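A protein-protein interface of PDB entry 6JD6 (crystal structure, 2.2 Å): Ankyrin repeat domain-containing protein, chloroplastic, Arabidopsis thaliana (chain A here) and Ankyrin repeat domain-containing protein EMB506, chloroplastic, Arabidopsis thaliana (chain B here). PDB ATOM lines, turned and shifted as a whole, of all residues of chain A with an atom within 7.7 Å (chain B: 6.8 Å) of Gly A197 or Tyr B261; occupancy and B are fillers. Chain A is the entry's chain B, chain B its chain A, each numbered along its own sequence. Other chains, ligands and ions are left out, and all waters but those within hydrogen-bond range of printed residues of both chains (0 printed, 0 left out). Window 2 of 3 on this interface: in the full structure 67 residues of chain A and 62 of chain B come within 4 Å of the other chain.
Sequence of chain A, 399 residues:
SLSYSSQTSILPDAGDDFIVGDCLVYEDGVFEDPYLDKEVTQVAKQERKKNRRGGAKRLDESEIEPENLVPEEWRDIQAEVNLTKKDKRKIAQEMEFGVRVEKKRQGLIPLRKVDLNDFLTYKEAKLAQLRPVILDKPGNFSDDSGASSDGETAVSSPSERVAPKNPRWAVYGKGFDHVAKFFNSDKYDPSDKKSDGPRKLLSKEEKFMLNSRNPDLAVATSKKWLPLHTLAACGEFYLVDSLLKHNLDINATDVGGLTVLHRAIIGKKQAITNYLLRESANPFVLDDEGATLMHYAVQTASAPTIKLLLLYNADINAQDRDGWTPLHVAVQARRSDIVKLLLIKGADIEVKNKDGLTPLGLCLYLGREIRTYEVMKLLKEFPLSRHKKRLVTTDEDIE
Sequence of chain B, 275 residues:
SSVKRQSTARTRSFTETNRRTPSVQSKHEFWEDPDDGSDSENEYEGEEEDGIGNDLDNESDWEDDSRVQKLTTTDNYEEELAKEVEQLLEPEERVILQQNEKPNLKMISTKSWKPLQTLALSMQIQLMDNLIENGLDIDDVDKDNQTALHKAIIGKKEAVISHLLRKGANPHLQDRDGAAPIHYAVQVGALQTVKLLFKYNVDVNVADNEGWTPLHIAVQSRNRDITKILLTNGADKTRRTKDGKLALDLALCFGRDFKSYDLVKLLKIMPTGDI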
ATOM      1  N   ASP A 196       8.405  10.154 -14.014  1.00  0.00           N
ATOM      2  CA  ASP A 196       7.756  10.704 -15.199  1.00  0.00           C
ATOM      3  C   ASP A 196       8.794  11.146 -16.229  1.00  0.00           C
ATOM      4  O   ASP A 196       9.448  10.314 -16.860  1.00  0.00           O
ATOM      5  CB  ASP A 196       6.838  11.870 -14.811  1.00  0.00           C
ATOM      6  CG  ASP A 196       6.001  12.376 -15.976  1.00  0.00           C
ATOM      7  OD1 ASP A 196       5.695  13.588 -16.002  1.00  0.00           O
ATOM      8  OD2 ASP A 196       5.655  11.567 -16.863  1.00  0.00           O
ATOM      9  N   GLY A 197       8.949  12.457 -16.391  1.00  0.00           N
ATOM     10  CA  GLY A 197       9.886  13.002 -17.355  1.00  0.00           C
ATOM     11  C   GLY A 197      11.302  13.031 -16.819  1.00  0.00           C
ATOM     12  O   GLY A 197      12.116  12.184 -17.172  1.00  0.00           O
ATOM     13  N   PRO A 198      11.605  14.013 -15.959  1.00  0.00           N
ATOM     14  CA  PRO A 198      12.929  14.186 -15.349  1.00  0.00           C
ATOM     15  C   PRO A 198      13.396  12.989 -14.521  1.00  0.00           C
ATOM     16  O   PRO A 198      14.599  12.826 -14.331  1.00  0.00           O
ATOM     17  CB  PRO A 198      12.732  15.405 -14.445  1.00  0.00           C
ATOM     18  CG  PRO A 198      11.652  16.176 -15.111  1.00  0.00           C
ATOM     19  CD  PRO A 198      10.709  15.140 -15.645  1.00  0.00           C
ATOM     20  N   ARG A 199      12.469  12.172 -14.035  1.00  0.00           N
ATOM     21  CA  ARG A 199      12.832  11.001 -13.240  1.00  0.00           C
ATOM     22  C   ARG A 199      13.703  10.024 -14.040  1.00  0.00           C
ATOM     23  O   ARG A 199      14.538   9.315 -13.476  1.00  0.00           O
ATOM     24  CB  ARG A 199      11.574  10.304 -12.705  1.00  0.00           C
ATOM     25  CG  ARG A 199      11.845   9.116 -11.790  1.00  0.00           C
ATOM     26  CD  ARG A 199      10.562   8.599 -11.152  1.00  0.00           C
ATOM     27  NE  ARG A 199       9.973   9.581 -10.244  1.00  0.00           N
ATOM     28  CZ  ARG A 199       8.910   9.353  -9.479  1.00  0.00           C
ATOM     29  NH1 ARG A 199       8.309   8.172  -9.507  1.00  0.00           N
ATOM     30  NH2 ARG A 199       8.449  10.309  -8.684  1.00  0.00           N
ATOM     31  N   LYS A 200      13.517  10.001 -15.357  1.00  0.00           N
ATOM     32  CA  LYS A 200      14.315   9.136 -16.223  1.00  0.00           C
ATOM     33  C   LYS A 200      15.740   9.667 -16.371  1.00  0.00           C
ATOM     34  O   LYS A 200      16.628   8.953 -16.830  1.00  0.00           O
ATOM     35  CB  LYS A 200      13.665   9.005 -17.601  1.00  0.00           C
ATOM     36  CG  LYS A 200      13.955  10.178 -18.523  1.00  0.00           C
ATOM     37  CD  LYS A 200      12.974  10.244 -19.682  1.00  0.00           C
ATOM     38  CE  LYS A 200      12.980  11.629 -20.316  1.00  0.00           C
ATOM     39  NZ  LYS A 200      14.359  12.075 -20.665  1.00  0.00           N
ATOM     40  N   LEU A 201      15.950  10.924 -15.985  1.00  0.00           N
ATOM     41  CA  LEU A 201      17.272  11.543 -16.057  1.00  0.00           C
ATOM     42  C   LEU A 201      18.131  11.152 -14.857  1.00  0.00           C
ATOM     43  O   LEU A 201      19.321  11.474 -14.795  1.00  0.00           O
ATOM     44  CB  LEU A 201      17.151  13.069 -16.137  1.00  0.00           C
ATOM     45  CG  LEU A 201      16.539  13.637 -17.422  1.00  0.00           C
ATOM     46  CD1 LEU A 201      16.483  15.152 -17.372  1.00  0.00           C
ATOM     47  CD2 LEU A 201      17.319  13.162 -18.647  1.00  0.00           C
ATOM     48  N   LEU A 202      17.517  10.458 -13.906  1.00  0.00           N
ATOM     49  CA  LEU A 202      18.186  10.108 -12.659  1.00  0.00           C
ATOM     50  C   LEU A 202      18.832   8.738 -12.744  1.00  0.00           C
ATOM     51  O   LEU A 202      18.349   7.855 -13.452  1.00  0.00           O
ATOM     52  CB  LEU A 202      17.189  10.127 -11.503  1.00  0.00           C
ATOM     53  CG  LEU A 202      16.505  11.460 -11.216  1.00  0.00           C
ATOM     54  CD1 LEU A 202      15.475  11.287 -10.118  1.00  0.00           C
ATOM     55  CD2 LEU A 202      17.543  12.500 -10.828  1.00  0.00           C
ATOM     56  N   LEU A 210      15.101   9.405  -4.161  1.00  0.00           N
ATOM     57  CA  LEU A 210      13.868  10.149  -4.375  1.00  0.00           C
ATOM     58  C   LEU A 210      12.665   9.419  -3.785  1.00  0.00           C
ATOM     59  O   LEU A 210      11.738  10.044  -3.264  1.00  0.00           O
ATOM     60  CB  LEU A 210      13.654  10.382  -5.872  1.00  0.00           C
ATOM     61  CG  LEU A 210      12.469  11.262  -6.265  1.00  0.00           C
ATOM     62  CD1 LEU A 210      12.539  12.603  -5.538  1.00  0.00           C
ATOM     63  CD2 LEU A 210      12.432  11.468  -7.772  1.00  0.00           C
ATOM     64  N   ARG B 222      13.150  23.983   0.259  1.00  0.00           N
ATOM     65  CA  ARG B 222      12.094  23.330  -0.535  1.00  0.00           C
ATOM     66  C   ARG B 222      11.233  24.314  -1.322  1.00  0.00           C
ATOM     67  O   ARG B 222      10.165  23.949  -1.821  1.00  0.00           O
ATOM     68  CB  ARG B 222      11.194  22.415   0.320  1.00  0.00           C
ATOM     69  CG  ARG B 222      11.924  21.580   1.374  1.00  0.00           C
ATOM     70  CD  ARG B 222      13.148  20.897   0.788  1.00  0.00           C
ATOM     71  NE  ARG B 222      12.822  19.737  -0.036  1.00  0.00           N
ATOM     72  CZ  ARG B 222      13.709  19.102  -0.794  1.00  0.00           C
ATOM     73  NH1 ARG B 222      14.959  19.546  -0.855  1.00  0.00           N
ATOM     74  NH2 ARG B 222      13.350  18.038  -1.498  1.00  0.00           N
ATOM     75  N   ALA B 251      17.885  18.259  -3.388  1.00  0.00           N
ATOM     76  CA  ALA B 251      16.513  18.029  -3.824  1.00  0.00           C
ATOM     77  C   ALA B 251      16.112  16.580  -3.579  1.00  0.00           C
ATOM     78  O   ALA B 251      15.017  16.305  -3.093  1.00  0.00           O
ATOM     79  CB  ALA B 251      16.352  18.384  -5.301  1.00  0.00           C
ATOM     80  N   GLY B 255      13.742  12.655   0.043  1.00  0.00           N
ATOM     81  CA  GLY B 255      12.840  11.589  -0.361  1.00  0.00           C
ATOM     82  C   GLY B 255      11.441  12.133  -0.595  1.00  0.00           C
ATOM     83  O   GLY B 255      11.273  13.324  -0.859  1.00  0.00           O
ATOM     84  N   ARG B 256      10.433  11.272  -0.488  1.00  0.00           N
ATOM     85  CA  ARG B 256       9.058  11.689  -0.755  1.00  0.00           C
ATOM     86  C   ARG B 256       8.495  12.669   0.285  1.00  0.00           C
ATOM     87  O   ARG B 256       9.045  12.820   1.378  1.00  0.00           O
ATOM     88  CB  ARG B 256       8.145  10.468  -0.889  1.00  0.00           C
ATOM     89  CG  ARG B 256       8.351   9.411   0.177  1.00  0.00           C
ATOM     90  CD  ARG B 256       7.286   8.327   0.085  1.00  0.00           C
ATOM     91  NE  ARG B 256       7.210   7.733  -1.248  1.00  0.00           N
ATOM     92  CZ  ARG B 256       7.654   6.517  -1.557  1.00  0.00           C
ATOM     93  NH1 ARG B 256       8.205   5.753  -0.625  1.00  0.00           N
ATOM     94  NH2 ARG B 256       7.540   6.062  -2.797  1.00  0.00           N
ATOM     95  N   PHE B 258       8.383  15.913   0.489  1.00  0.00           N
ATOM     96  CA  PHE B 258       9.069  17.174   0.740  1.00  0.00           C
ATOM     97  C   PHE B 258       9.234  17.970  -0.552  1.00  0.00           C
ATOM     98  O   PHE B 258      10.202  18.717  -0.707  1.00  0.00           O
ATOM     99  CB  PHE B 258      10.443  16.935   1.380  1.00  0.00           C
ATOM    100  CG  PHE B 258      10.385  16.627   2.852  1.00  0.00           C
ATOM    101  CD1 PHE B 258      10.474  17.642   3.788  1.00  0.00           C
ATOM    102  CD2 PHE B 258      10.245  15.324   3.297  1.00  0.00           C
ATOM    103  CE1 PHE B 258      10.421  17.363   5.143  1.00  0.00           C
ATOM    104  CE2 PHE B 258      10.195  15.040   4.650  1.00  0.00           C
ATOM    105  CZ  PHE B 258      10.282  16.058   5.571  1.00  0.00           C
ATOM    106  N   LYS B 259       8.292  17.790  -1.475  1.00  0.00           N
ATOM    107  CA  LYS B 259       8.310  18.468  -2.770  1.00  0.00           C
ATOM    108  C   LYS B 259       9.575  18.143  -3.563  1.00  0.00           C
ATOM    109  O   LYS B 259      10.017  18.928  -4.400  1.00  0.00           O
ATOM    110  CB  LYS B 259       8.146  19.983  -2.585  1.00  0.00           C
ATOM    111  CG  LYS B 259       6.783  20.372  -2.017  1.00  0.00           C
ATOM    112  CD  LYS B 259       6.889  21.486  -0.994  1.00  0.00           C
ATOM    113  CE  LYS B 259       7.203  22.813  -1.650  1.00  0.00           C
ATOM    114  NZ  LYS B 259       7.548  23.843  -0.631  1.00  0.00           N
ATOM    115  N   SER B 260      10.140  16.969  -3.300  1.00  0.00           N
ATOM    116  CA  SER B 260      11.427  16.590  -3.867  1.00  0.00           C
ATOM    117  C   SER B 260      11.384  16.435  -5.379  1.00  0.00           C
ATOM    118  O   SER B 260      12.284  16.899  -6.078  1.00  0.00           O
ATOM    119  CB  SER B 260      11.936  15.303  -3.225  1.00  0.00           C
ATOM    120  OG  SER B 260      12.172  15.499  -1.843  1.00  0.00           O
ATOM    121  N   TYR B 261      10.345  15.781  -5.887  1.00  0.00           N
ATOM    122  CA  TYR B 261      10.240  15.563  -7.321  1.00  0.00           C
ATOM    123  C   TYR B 261      10.097  16.873  -8.096  1.00  0.00           C
ATOM    124  O   TYR B 261      10.697  17.037  -9.153  1.00  0.00           O
ATOM    125  CB  TYR B 261       9.087  14.620  -7.669  1.00  0.00           C
ATOM    126  CG  TYR B 261       9.032  14.323  -9.149  1.00  0.00           C
ATOM    127  CD1 TYR B 261       9.943  13.453  -9.729  1.00  0.00           C
ATOM    128  CD2 TYR B 261       8.094  14.934  -9.971  1.00  0.00           C
ATOM    129  CE1 TYR B 261       9.914  13.186 -11.082  1.00  0.00           C
ATOM    130  CE2 TYR B 261       8.055  14.669 -11.329  1.00  0.00           C
ATOM    131  CZ  TYR B 261       8.970  13.794 -11.876  1.00  0.00           C
ATOM    132  OH  TYR B 261       8.951  13.522 -13.224  1.00  0.00           O
ATOM    133  N   ASP B 262       9.300  17.797  -7.569  1.00  0.00           N
ATOM    134  CA  ASP B 262       9.117  19.092  -8.214  1.00  0.00           C
ATOM    135  C   ASP B 262      10.432  19.851  -8.307  1.00  0.00           C
ATOM    136  O   ASP B 262      10.743  20.446  -9.339  1.00  0.00           O
ATOM    137  CB  ASP B 262       8.086  19.939  -7.466  1.00  0.00           C
ATOM    138  CG  ASP B 262       6.671  19.444  -7.670  1.00  0.00           C
ATOM    139  OD1 ASP B 262       6.442  18.679  -8.631  1.00  0.00           O
ATOM    140  OD2 ASP B 262       5.788  19.825  -6.874  1.00  0.00           O
ATOM    141  N   LEU B 263      11.199  19.827  -7.222  1.00  0.00           N
ATOM    142  CA  LEU B 263      12.495  20.492  -7.190  1.00  0.00           C
ATOM    143  C   LEU B 263      13.480  19.858  -8.178  1.00  0.00           C
ATOM    144  O   LEU B 263      14.193  20.566  -8.894  1.00  0.00           O
ATOM    145  CB  LEU B 263      13.060  20.492  -5.767  1.00  0.00           C
ATOM    146  CG  LEU B 263      12.292  21.397  -4.796  1.00  0.00           C
ATOM    147  CD1 LEU B 263      12.670  21.102  -3.359  1.00  0.00           C
ATOM    148  CD2 LEU B 263      12.530  22.871  -5.118  1.00  0.00           C
ATOM    149  N   VAL B 264      13.506  18.528  -8.218  1.00  0.00           N
ATOM    150  CA  VAL B 264      14.356  17.799  -9.157  1.00  0.00           C
ATOM    151  C   VAL B 264      14.013  18.185 -10.593  1.00  0.00           C
ATOM    152  O   VAL B 264      14.896  18.416 -11.420  1.00  0.00           O
ATOM    153  CB  VAL B 264      14.203  16.270  -8.985  1.00  0.00           C
ATOM    154  CG1 VAL B 264      14.722  15.522 -10.217  1.00  0.00           C
ATOM    155  CG2 VAL B 264      14.917  15.803  -7.727  1.00  0.00           C
ATOM    156  N   LYS B 265      12.718  18.267 -10.872  1.00  0.00           N
ATOM    157  CA  LYS B 265      12.227  18.643 -12.190  1.00  0.00           C
ATOM    158  C   LYS B 265      12.734  20.030 -12.595  1.00  0.00           C
ATOM    159  O   LYS B 265      13.263  20.205 -13.688  1.00  0.00           O
ATOM    160  CB  LYS B 265      10.700  18.579 -12.203  1.00  0.00           C
ATOM    161  CG  LYS B 265      10.053  18.853 -13.539  1.00  0.00           C
ATOM    162  CD  LYS B 265       8.703  18.152 -13.636  1.00  0.00           C
ATOM    163  CE  LYS B 265       7.819  18.467 -12.432  1.00  0.00           C
ATOM    164  NZ  LYS B 265       6.466  17.848 -12.557  1.00  0.00           N
ATOM    165  N   LEU B 266      12.589  21.005 -11.703  1.00  0.00           N
ATOM    166  CA  LEU B 266      13.130  22.342 -11.927  1.00  0.00           C
ATOM    167  C   LEU B 266      14.632  22.316 -12.206  1.00  0.00           C
ATOM    168  O   LEU B 266      15.125  23.037 -13.072  1.00  0.00           O
ATOM    169  CB  LEU B 266      12.860  23.241 -10.718  1.00  0.00           C
ATOM    170  CG  LEU B 266      11.429  23.743 -10.524  1.00  0.00           C
ATOM    171  CD1 LEU B 266      11.309  24.516  -9.219  1.00  0.00           C
ATOM    172  CD2 LEU B 266      11.005  24.606 -11.704  1.00  0.00           C
ATOM    173  N   ILE B 269      15.442  20.847 -15.783  1.00  0.00           N
ATOM    174  CA  ILE B 269      14.894  21.535 -16.948  1.00  0.00           C
ATOM    175  C   ILE B 269      15.310  23.008 -17.035  1.00  0.00           C
ATOM    176  O   ILE B 269      15.742  23.469 -18.089  1.00  0.00           O
ATOM    177  CB  ILE B 269      13.361  21.414 -16.983  1.00  0.00           C
ATOM    178  CG1 ILE B 269      12.960  19.943 -17.103  1.00  0.00           C
ATOM    179  CG2 ILE B 269      12.785  22.219 -18.133  1.00  0.00           C
ATOM    180  CD1 ILE B 269      11.468  19.706 -17.027  1.00  0.00           C
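Among the printed residues, merely in contact across the chains: Asp A196 with Tyr B261 (3.1 Å), Pro A198 with Tyr B261 (3.4 Å), Leu A210 with Gly B255 (3.4 Å), Pro A198 with Lys B265 (3.5 Å), Leu A210 with Ser B260 (3.6 Å), Arg A199 with Tyr B261 (3.6 Å) and Leu A210 with Tyr B261 (3.7 Å).
Gly A197 touches just one residue of chain B: Tyr B261.
Printed residues of chain A within 4 Å of Lys B265: Pro A198.
Of the printed residues of chain B, Arg A199 touches Tyr B261.
Printed residues of chain B within 4 Å of Asp A196: Tyr B261 (3.1 Å).
Printed residues of chain A within 4 Å of Gly B255: Leu A210 (3.4 Å).
Of the printed residues of chain B, Pro A198 touches Tyr B261 and Lys B265.
Leu B266 touches none of the printed residues of chain A.
The nearest residue of chain A that does not touch Tyr B261 is Leu A202 (6.0 Å).
The nearest printed residue of chain B that does not touch Leu A210 is Val B264 (4.5 Å).
O of Gly B255 is in hydrogen-bond range of OG of Ser B260, 2.6 Å away.
The guanidinium group (NH2) of Arg B222 is in hydrogen-bond range of the side-chain hydroxyl (OG) of Ser B260, 2.8 Å away.
The side-chain hydroxyl (OG) of Ser B260 lies within hydrogen-bond range of the backbone carbonyl oxygen (O) of Ala B251 (3.2 Å).
Of the 14 printed residues of chain B, 5 touch a printed residue of chain A.
Hydrophobic or aromatic side chains of chain B that line the printed part of chain A: Tyr B261.
Hydrophobic or aromatic side chains of chain A within 4 Å of the printed part of chain B: Pro A198 and Leu A210.
Along chain A the printed residues that touch a printed residue of chain B span positions 196 to 210.
The side-chain hydroxyl of Tyr B261 sits at hydrogen-bond distance from the backbone NH of Gly A197, at 3.3 Å.
The backbone NH (N) of Arg B256 lies within hydrogen-bond range of the backbone carbonyl oxygen (O) of Leu A210, 3.3 Å away.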
